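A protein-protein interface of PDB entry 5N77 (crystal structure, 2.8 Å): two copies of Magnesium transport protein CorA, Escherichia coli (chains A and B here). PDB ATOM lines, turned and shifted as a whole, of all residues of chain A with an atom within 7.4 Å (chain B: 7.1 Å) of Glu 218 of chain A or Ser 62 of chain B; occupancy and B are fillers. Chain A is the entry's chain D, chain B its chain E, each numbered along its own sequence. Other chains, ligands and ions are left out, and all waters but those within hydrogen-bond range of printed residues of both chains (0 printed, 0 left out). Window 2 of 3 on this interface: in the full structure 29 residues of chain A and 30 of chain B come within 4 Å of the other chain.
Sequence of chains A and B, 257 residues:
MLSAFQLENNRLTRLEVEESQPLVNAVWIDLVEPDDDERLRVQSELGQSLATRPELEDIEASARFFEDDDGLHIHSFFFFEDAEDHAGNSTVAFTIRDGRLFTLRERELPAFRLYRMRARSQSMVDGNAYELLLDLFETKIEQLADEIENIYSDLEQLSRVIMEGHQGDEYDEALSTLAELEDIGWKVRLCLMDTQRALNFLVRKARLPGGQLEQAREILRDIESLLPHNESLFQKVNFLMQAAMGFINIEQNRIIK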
ATOM      1  N   GLU A 138     -14.707 -29.268   6.491  1.00  0.00           N
ATOM      2  CA  GLU A 138     -13.721 -29.423   7.570  1.00  0.00           C
ATOM      3  C   GLU A 138     -12.356 -29.781   7.001  1.00  0.00           C
ATOM      4  O   GLU A 138     -11.332 -29.226   7.406  1.00  0.00           O
ATOM      5  CB  GLU A 138     -14.125 -30.532   8.541  1.00  0.00           C
ATOM      6  CG  GLU A 138     -14.674 -30.066   9.871  1.00  0.00           C
ATOM      7  CD  GLU A 138     -15.229 -31.214  10.699  1.00  0.00           C
ATOM      8  OE1 GLU A 138     -16.392 -31.123  11.161  1.00  0.00           O
ATOM      9  OE2 GLU A 138     -14.514 -32.220  10.878  1.00  0.00           O
ATOM     10  N   ILE A 141     -10.694 -26.948   5.050  1.00  0.00           N
ATOM     11  CA  ILE A 141     -10.100 -25.952   5.968  1.00  0.00           C
ATOM     12  C   ILE A 141      -8.807 -26.493   6.565  1.00  0.00           C
ATOM     13  O   ILE A 141      -7.828 -25.787   6.688  1.00  0.00           O
ATOM     14  CB  ILE A 141     -11.095 -25.502   7.089  1.00  0.00           C
ATOM     15  CG1 ILE A 141     -11.878 -24.254   6.685  1.00  0.00           C
ATOM     16  CG2 ILE A 141     -10.357 -25.111   8.363  1.00  0.00           C
ATOM     17  CD1 ILE A 141     -12.607 -24.357   5.374  1.00  0.00           C
ATOM     18  N   LEU A 199     -21.189 -21.538   4.013  1.00  0.00           N
ATOM     19  CA  LEU A 199     -21.623 -21.919   5.357  1.00  0.00           C
ATOM     20  C   LEU A 199     -22.603 -20.916   5.985  1.00  0.00           C
ATOM     21  O   LEU A 199     -23.509 -21.332   6.683  1.00  0.00           O
ATOM     22  CB  LEU A 199     -20.437 -22.099   6.282  1.00  0.00           C
ATOM     23  CG  LEU A 199     -19.571 -23.301   5.934  1.00  0.00           C
ATOM     24  CD1 LEU A 199     -18.262 -23.187   6.681  1.00  0.00           C
ATOM     25  CD2 LEU A 199     -20.217 -24.620   6.281  1.00  0.00           C
ATOM     26  N   GLN A 212     -25.109 -31.037  13.311  1.00  0.00           N
ATOM     27  CA  GLN A 212     -24.571 -30.399  12.110  1.00  0.00           C
ATOM     28  C   GLN A 212     -24.411 -28.895  12.262  1.00  0.00           C
ATOM     29  O   GLN A 212     -23.491 -28.322  11.701  1.00  0.00           O
ATOM     30  CB  GLN A 212     -25.458 -30.689  10.896  1.00  0.00           C
ATOM     31  CG  GLN A 212     -25.106 -31.978  10.185  1.00  0.00           C
ATOM     32  CD  GLN A 212     -25.292 -33.191  11.066  1.00  0.00           C
ATOM     33  OE1 GLN A 212     -26.335 -33.849  11.016  1.00  0.00           O
ATOM     34  NE2 GLN A 212     -24.280 -33.499  11.875  1.00  0.00           N
ATOM     35  N   LEU A 213     -25.322 -28.256  12.990  1.00  0.00           N
ATOM     36  CA  LEU A 213     -25.280 -26.809  13.156  1.00  0.00           C
ATOM     37  C   LEU A 213     -24.038 -26.373  13.903  1.00  0.00           C
ATOM     38  O   LEU A 213     -23.384 -25.401  13.522  1.00  0.00           O
ATOM     39  CB  LEU A 213     -26.516 -26.306  13.890  1.00  0.00           C
ATOM     40  CG  LEU A 213     -26.713 -24.789  13.832  1.00  0.00           C
ATOM     41  CD1 LEU A 213     -26.889 -24.335  12.393  1.00  0.00           C
ATOM     42  CD2 LEU A 213     -27.908 -24.369  14.678  1.00  0.00           C
ATOM     43  N   GLU A 214     -23.714 -27.087  14.973  1.00  0.00           N
ATOM     44  CA  GLU A 214     -22.524 -26.770  15.758  1.00  0.00           C
ATOM     45  C   GLU A 214     -21.249 -27.008  14.913  1.00  0.00           C
ATOM     46  O   GLU A 214     -20.292 -26.229  14.967  1.00  0.00           O
ATOM     47  CB  GLU A 214     -22.514 -27.574  17.071  1.00  0.00           C
ATOM     48  CG  GLU A 214     -21.322 -27.312  18.002  1.00  0.00           C
ATOM     49  CD  GLU A 214     -20.926 -25.835  18.127  1.00  0.00           C
ATOM     50  OE1 GLU A 214     -21.727 -25.014  18.638  1.00  0.00           O
ATOM     51  OE2 GLU A 214     -19.795 -25.477  17.704  1.00  0.00           O
ATOM     52  N   GLN A 215     -21.265 -28.078  14.123  1.00  0.00           N
ATOM     53  CA  GLN A 215     -20.159 -28.414  13.221  1.00  0.00           C
ATOM     54  C   GLN A 215     -19.873 -27.273  12.256  1.00  0.00           C
ATOM     55  O   GLN A 215     -18.725 -26.881  12.066  1.00  0.00           O
ATOM     56  CB  GLN A 215     -20.527 -29.660  12.432  1.00  0.00           C
ATOM     57  CG  GLN A 215     -19.417 -30.285  11.627  1.00  0.00           C
ATOM     58  CD  GLN A 215     -19.849 -31.599  10.986  1.00  0.00           C
ATOM     59  OE1 GLN A 215     -20.988 -32.028  11.127  1.00  0.00           O
ATOM     60  NE2 GLN A 215     -18.953 -32.200  10.219  1.00  0.00           N
ATOM     61  N   ALA A 216     -20.934 -26.760  11.656  1.00  0.00           N
ATOM     62  CA  ALA A 216     -20.847 -25.643  10.750  1.00  0.00           C
ATOM     63  C   ALA A 216     -20.276 -24.399  11.432  1.00  0.00           C
ATOM     64  O   ALA A 216     -19.443 -23.694  10.854  1.00  0.00           O
ATOM     65  CB  ALA A 216     -22.218 -25.332  10.169  1.00  0.00           C
ATOM     66  N   ARG A 217     -20.748 -24.110  12.639  1.00  0.00           N
ATOM     67  CA  ARG A 217     -20.265 -22.942  13.365  1.00  0.00           C
ATOM     68  C   ARG A 217     -18.792 -23.094  13.687  1.00  0.00           C
ATOM     69  O   ARG A 217     -18.043 -22.137  13.642  1.00  0.00           O
ATOM     70  CB  ARG A 217     -21.057 -22.723  14.645  1.00  0.00           C
ATOM     71  CG  ARG A 217     -22.500 -22.309  14.413  1.00  0.00           C
ATOM     72  CD  ARG A 217     -23.097 -21.658  15.661  1.00  0.00           C
ATOM     73  NE  ARG A 217     -24.432 -21.100  15.403  1.00  0.00           N
ATOM     74  CZ  ARG A 217     -25.584 -21.578  15.879  1.00  0.00           C
ATOM     75  NH1 ARG A 217     -25.614 -22.637  16.687  1.00  0.00           N
ATOM     76  NH2 ARG A 217     -26.722 -20.981  15.545  1.00  0.00           N
ATOM     77  N   GLU A 218     -18.381 -24.313  13.998  1.00  0.00           N
ATOM     78  CA  GLU A 218     -16.977 -24.600  14.273  1.00  0.00           C
ATOM     79  C   GLU A 218     -16.102 -24.291  13.052  1.00  0.00           C
ATOM     80  O   GLU A 218     -15.034 -23.684  13.165  1.00  0.00           O
ATOM     81  CB  GLU A 218     -16.811 -26.043  14.746  1.00  0.00           C
ATOM     82  CG  GLU A 218     -15.391 -26.483  14.993  1.00  0.00           C
ATOM     83  CD  GLU A 218     -15.245 -27.883  15.581  1.00  0.00           C
ATOM     84  OE1 GLU A 218     -16.227 -28.588  15.971  1.00  0.00           O
ATOM     85  OE2 GLU A 218     -14.091 -28.298  15.653  1.00  0.00           O
ATOM     86  N   ILE A 219     -16.581 -24.668  11.878  1.00  0.00           N
ATOM     87  CA  ILE A 219     -15.868 -24.373  10.642  1.00  0.00           C
ATOM     88  C   ILE A 219     -15.853 -22.869  10.385  1.00  0.00           C
ATOM     89  O   ILE A 219     -14.829 -22.307   9.997  1.00  0.00           O
ATOM     90  CB  ILE A 219     -16.479 -25.095   9.430  1.00  0.00           C
ATOM     91  CG1 ILE A 219     -16.425 -26.606   9.607  1.00  0.00           C
ATOM     92  CG2 ILE A 219     -15.708 -24.753   8.164  1.00  0.00           C
ATOM     93  CD1 ILE A 219     -17.177 -27.366   8.533  1.00  0.00           C
ATOM     94  N   LEU A 220     -16.985 -22.209  10.606  1.00  0.00           N
ATOM     95  CA  LEU A 220     -17.033 -20.748  10.477  1.00  0.00           C
ATOM     96  C   LEU A 220     -16.036 -20.086  11.402  1.00  0.00           C
ATOM     97  O   LEU A 220     -15.339 -19.165  10.998  1.00  0.00           O
ATOM     98  CB  LEU A 220     -18.428 -20.208  10.746  1.00  0.00           C
ATOM     99  CG  LEU A 220     -19.343 -20.241   9.521  1.00  0.00           C
ATOM    100  CD1 LEU A 220     -20.802 -20.027   9.890  1.00  0.00           C
ATOM    101  CD2 LEU A 220     -18.921 -19.166   8.531  1.00  0.00           C
ATOM    102  N   ARG A 221     -15.944 -20.575  12.631  1.00  0.00           N
ATOM    103  CA  ARG A 221     -14.993 -20.039  13.607  1.00  0.00           C
ATOM    104  C   ARG A 221     -13.552 -20.218  13.118  1.00  0.00           C
ATOM    105  O   ARG A 221     -12.692 -19.370  13.370  1.00  0.00           O
ATOM    106  CB  ARG A 221     -15.149 -20.752  14.953  1.00  0.00           C
ATOM    107  CG  ARG A 221     -15.232 -19.842  16.177  1.00  0.00           C
ATOM    108  CD  ARG A 221     -15.614 -20.619  17.451  1.00  0.00           C
ATOM    109  NE  ARG A 221     -17.016 -21.082  17.467  1.00  0.00           N
ATOM    110  CZ  ARG A 221     -17.437 -22.359  17.524  1.00  0.00           C
ATOM    111  NH1 ARG A 221     -16.588 -23.398  17.582  1.00  0.00           N
ATOM    112  NH2 ARG A 221     -18.744 -22.612  17.520  1.00  0.00           N
ATOM    113  N   ASP A 222     -13.275 -21.350  12.472  1.00  0.00           N
ATOM    114  CA  ASP A 222     -11.915 -21.626  11.966  1.00  0.00           C
ATOM    115  C   ASP A 222     -11.568 -20.668  10.865  1.00  0.00           C
ATOM    116  O   ASP A 222     -10.468 -20.112  10.841  1.00  0.00           O
ATOM    117  CB  ASP A 222     -11.779 -23.051  11.441  1.00  0.00           C
ATOM    118  CG  ASP A 222     -11.506 -24.054  12.539  1.00  0.00           C
ATOM    119  OD1 ASP A 222     -11.320 -23.642  13.724  1.00  0.00           O
ATOM    120  OD2 ASP A 222     -11.485 -25.268  12.222  1.00  0.00           O
ATOM    121  N   ILE A 223     -12.515 -20.474   9.958  1.00  0.00           N
ATOM    122  CA  ILE A 223     -12.330 -19.526   8.888  1.00  0.00           C
ATOM    123  C   ILE A 223     -12.069 -18.123   9.439  1.00  0.00           C
ATOM    124  O   ILE A 223     -11.137 -17.447   9.002  1.00  0.00           O
ATOM    125  CB  ILE A 223     -13.531 -19.471   7.958  1.00  0.00           C
ATOM    126  CG1 ILE A 223     -13.650 -20.783   7.209  1.00  0.00           C
ATOM    127  CG2 ILE A 223     -13.362 -18.351   6.945  1.00  0.00           C
ATOM    128  CD1 ILE A 223     -14.879 -20.873   6.329  1.00  0.00           C
ATOM    129  N   GLU A 224     -12.879 -17.678  10.396  1.00  0.00           N
ATOM    130  CA  GLU A 224     -12.676 -16.347  10.970  1.00  0.00           C
ATOM    131  C   GLU A 224     -11.241 -16.240  11.515  1.00  0.00           C
ATOM    132  O   GLU A 224     -10.646 -15.170  11.488  1.00  0.00           O
ATOM    133  CB  GLU A 224     -13.706 -16.015  12.040  1.00  0.00           C
ATOM    134  CG  GLU A 224     -13.636 -14.584  12.569  1.00  0.00           C
ATOM    135  CD  GLU A 224     -14.322 -14.399  13.935  1.00  0.00           C
ATOM    136  OE1 GLU A 224     -15.048 -15.318  14.412  1.00  0.00           O
ATOM    137  OE2 GLU A 224     -14.121 -13.318  14.548  1.00  0.00           O
ATOM    138  N   SER A 225     -10.682 -17.355  11.985  1.00  0.00           N
ATOM    139  CA  SER A 225      -9.346 -17.346  12.576  1.00  0.00           C
ATOM    140  C   SER A 225      -8.227 -17.498  11.584  1.00  0.00           C
ATOM    141  O   SER A 225      -7.082 -17.274  11.937  1.00  0.00           O
ATOM    142  CB  SER A 225      -9.199 -18.457  13.597  1.00  0.00           C
ATOM    143  OG  SER A 225      -8.838 -19.656  12.967  1.00  0.00           O
ATOM    144  N   ILE B  59      -2.648 -23.906  13.216  1.00  0.00           N
ATOM    145  CA  ILE B  59      -2.995 -22.505  13.528  1.00  0.00           C
ATOM    146  C   ILE B  59      -4.502 -22.196  13.590  1.00  0.00           C
ATOM    147  O   ILE B  59      -4.918 -21.164  14.114  1.00  0.00           O
ATOM    148  CB  ILE B  59      -2.315 -21.524  12.528  1.00  0.00           C
ATOM    149  CG1 ILE B  59      -2.764 -21.774  11.082  1.00  0.00           C
ATOM    150  CG2 ILE B  59      -0.809 -21.629  12.622  1.00  0.00           C
ATOM    151  CD1 ILE B  59      -2.473 -20.605  10.158  1.00  0.00           C
ATOM    152  N   GLU B  60      -5.275 -23.031  12.922  1.00  0.00           N
ATOM    153  CA  GLU B  60      -6.757 -23.098  12.995  1.00  0.00           C
ATOM    154  C   GLU B  60      -7.298 -23.004  14.423  1.00  0.00           C
ATOM    155  O   GLU B  60      -6.877 -23.759  15.290  1.00  0.00           O
ATOM    156  CB  GLU B  60      -7.245 -24.407  12.310  1.00  0.00           C
ATOM    157  CG  GLU B  60      -6.088 -25.345  11.935  1.00  0.00           C
ATOM    158  CD  GLU B  60      -6.467 -26.784  11.822  1.00  0.00           C
ATOM    159  OE1 GLU B  60      -7.643 -27.110  12.071  1.00  0.00           O
ATOM    160  OE2 GLU B  60      -5.582 -27.610  11.482  1.00  0.00           O
ATOM    161  N   ALA B  61      -8.230 -22.083  14.663  1.00  0.00           N
ATOM    162  CA  ALA B  61      -8.844 -21.906  15.994  1.00  0.00           C
ATOM    163  C   ALA B  61      -9.245 -23.219  16.659  1.00  0.00           C
ATOM    164  O   ALA B  61      -8.949 -23.451  17.840  1.00  0.00           O
ATOM    165  CB  ALA B  61     -10.061 -21.007  15.907  1.00  0.00           C
ATOM    166  N   SER B  62      -9.894 -24.092  15.900  1.00  0.00           N
ATOM    167  CA  SER B  62     -10.372 -25.366  16.447  1.00  0.00           C
ATOM    168  C   SER B  62      -9.250 -26.351  16.834  1.00  0.00           C
ATOM    169  O   SER B  62      -9.488 -27.358  17.472  1.00  0.00           O
ATOM    170  CB  SER B  62     -11.280 -26.044  15.451  1.00  0.00           C
ATOM    171  OG  SER B  62     -10.539 -26.498  14.339  1.00  0.00           O
ATOM    172  N   ALA B  63      -8.022 -26.044  16.454  1.00  0.00           N
ATOM    173  CA  ALA B  63      -6.877 -26.855  16.805  1.00  0.00           C
ATOM    174  C   ALA B  63      -6.097 -26.246  17.928  1.00  0.00           C
ATOM    175  O   ALA B  63      -5.186 -26.872  18.417  1.00  0.00           O
ATOM    176  CB  ALA B  63      -5.967 -26.994  15.607  1.00  0.00           C
ATOM    177  N   ARG B  64      -6.435 -25.016  18.306  1.00  0.00           N
ATOM    178  CA  ARG B  64      -5.734 -24.265  19.343  1.00  0.00           C
ATOM    179  C   ARG B  64      -6.564 -23.956  20.595  1.00  0.00           C
ATOM    180  O   ARG B  64      -6.015 -23.840  21.680  1.00  0.00           O
ATOM    181  CB  ARG B  64      -5.350 -22.910  18.817  1.00  0.00           C
ATOM    182  CG  ARG B  64      -4.463 -22.889  17.609  1.00  0.00           C
ATOM    183  CD  ARG B  64      -3.698 -21.584  17.528  1.00  0.00           C
ATOM    184  NE  ARG B  64      -2.322 -21.909  17.263  1.00  0.00           N
ATOM    185  CZ  ARG B  64      -1.292 -21.321  17.835  1.00  0.00           C
ATOM    186  NH1 ARG B  64      -1.483 -20.360  18.711  1.00  0.00           N
ATOM    187  NH2 ARG B  64      -0.062 -21.685  17.520  1.00  0.00           N
ATOM    188  N   PHE B  65      -7.866 -23.742  20.438  1.00  0.00           N
ATOM    189  CA  PHE B  65      -8.724 -23.358  21.557  1.00  0.00           C
ATOM    190  C   PHE B  65      -9.922 -24.283  21.584  1.00  0.00           C
ATOM    191  O   PHE B  65     -10.873 -24.130  20.807  1.00  0.00           O
ATOM    192  CB  PHE B  65      -9.164 -21.918  21.407  1.00  0.00           C
ATOM    193  CG  PHE B  65      -8.059 -20.994  20.969  1.00  0.00           C
ATOM    194  CD1 PHE B  65      -6.929 -20.801  21.755  1.00  0.00           C
ATOM    195  CD2 PHE B  65      -8.153 -20.315  19.763  1.00  0.00           C
ATOM    196  CE1 PHE B  65      -5.912 -19.973  21.331  1.00  0.00           C
ATOM    197  CE2 PHE B  65      -7.143 -19.474  19.348  1.00  0.00           C
ATOM    198  CZ  PHE B  65      -6.017 -19.314  20.125  1.00  0.00           C
ATOM    199  N   PHE B  66      -9.838 -25.295  22.439  1.00  0.00           N
ATOM    200  CA  PHE B  66     -10.812 -26.376  22.440  1.00  0.00           C
ATOM    201  C   PHE B  66     -10.853 -27.135  23.760  1.00  0.00           C
ATOM    202  O   PHE B  66      -9.915 -27.083  24.546  1.00  0.00           O
ATOM    203  CB  PHE B  66     -10.544 -27.330  21.269  1.00  0.00           C
ATOM    204  CG  PHE B  66      -9.269 -28.115  21.384  1.00  0.00           C
ATOM    205  CD1 PHE B  66      -8.067 -27.546  21.048  1.00  0.00           C
ATOM    206  CD2 PHE B  66      -9.286 -29.434  21.785  1.00  0.00           C
ATOM    207  CE1 PHE B  66      -6.881 -28.267  21.151  1.00  0.00           C
ATOM    208  CE2 PHE B  66      -8.116 -30.165  21.882  1.00  0.00           C
ATOM    209  CZ  PHE B  66      -6.908 -29.578  21.572  1.00  0.00           C
ATOM    210  N   GLU B  67     -11.978 -27.799  23.999  1.00  0.00           N
ATOM    211  CA  GLU B  67     -12.220 -28.608  25.205  1.00  0.00           C
ATOM    212  C   GLU B  67     -12.500 -30.044  24.798  1.00  0.00           C
ATOM    213  O   GLU B  67     -13.210 -30.283  23.834  1.00  0.00           O
ATOM    214  CB  GLU B  67     -13.451 -28.117  25.966  1.00  0.00           C
ATOM    215  CG  GLU B  67     -13.205 -26.974  26.931  1.00  0.00           C
ATOM    216  CD  GLU B  67     -14.421 -26.687  27.794  1.00  0.00           C
ATOM    217  OE1 GLU B  67     -15.439 -26.222  27.238  1.00  0.00           O
ATOM    218  OE2 GLU B  67     -14.368 -26.947  29.014  1.00  0.00           O
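OG of Ser 62 of chain B is in hydrogen-bond range of OD2 of Asp 222 of chain A, at 2.6 Å.
The side-chain hydroxyl of Ser 225 of chain A sits at hydrogen-bond distance from the backbone NH of Ala 61 of chain B.
O of Asp 222 of chain A sits at hydrogen-bond distance from OG of Ser 225 of chain A, at 2.7 Å.
OE2 of Glu 218 of chain A touches CB of Ser 62 of chain B, 3.6 Å away.
Asp 222 of chain A touches Ala 61 of chain B (OD1 to N, 3.6 Å).
Glu 60 of chain B touches Ser 225 of chain A.
Of chain B, only Ser 62 comes within 4 Å of Glu 218 of chain A.
Of the printed residues of chain B, Asp 222 of chain A touches Ala 61 and Ser 62.
Of the printed residues of chain B, Ser 225 of chain A touches Glu 60 (3.96 Å) and Ala 61 (3.0 Å).
Of the printed residues of chain A, Glu 60 of chain B touches Ser 225.
Printed residues of chain A within 4 Å of Ala 61 of chain B: Asp 222 (3.6 Å) and Ser 225 (3.0 Å).
Of chain A, only Glu 218 (3.6 Å) and Asp 222 (2.6 Å) come within 4 Å of Ser 62 of chain B.
The nearest residue of chain B that does not touch Glu 218 of chain A is Ala 61 of chain B (6.3 Å).
Of the 9 printed residues of chain B, 3 touch a printed residue of chain A.
Hydrophobic or aromatic side chains of chain B that line the printed part of chain A: Ala 61.
No position is printed for both chains.
Of the 5 pairs that touch across the chains among the printed residues, none has its exchanged pair printed and touching as well.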
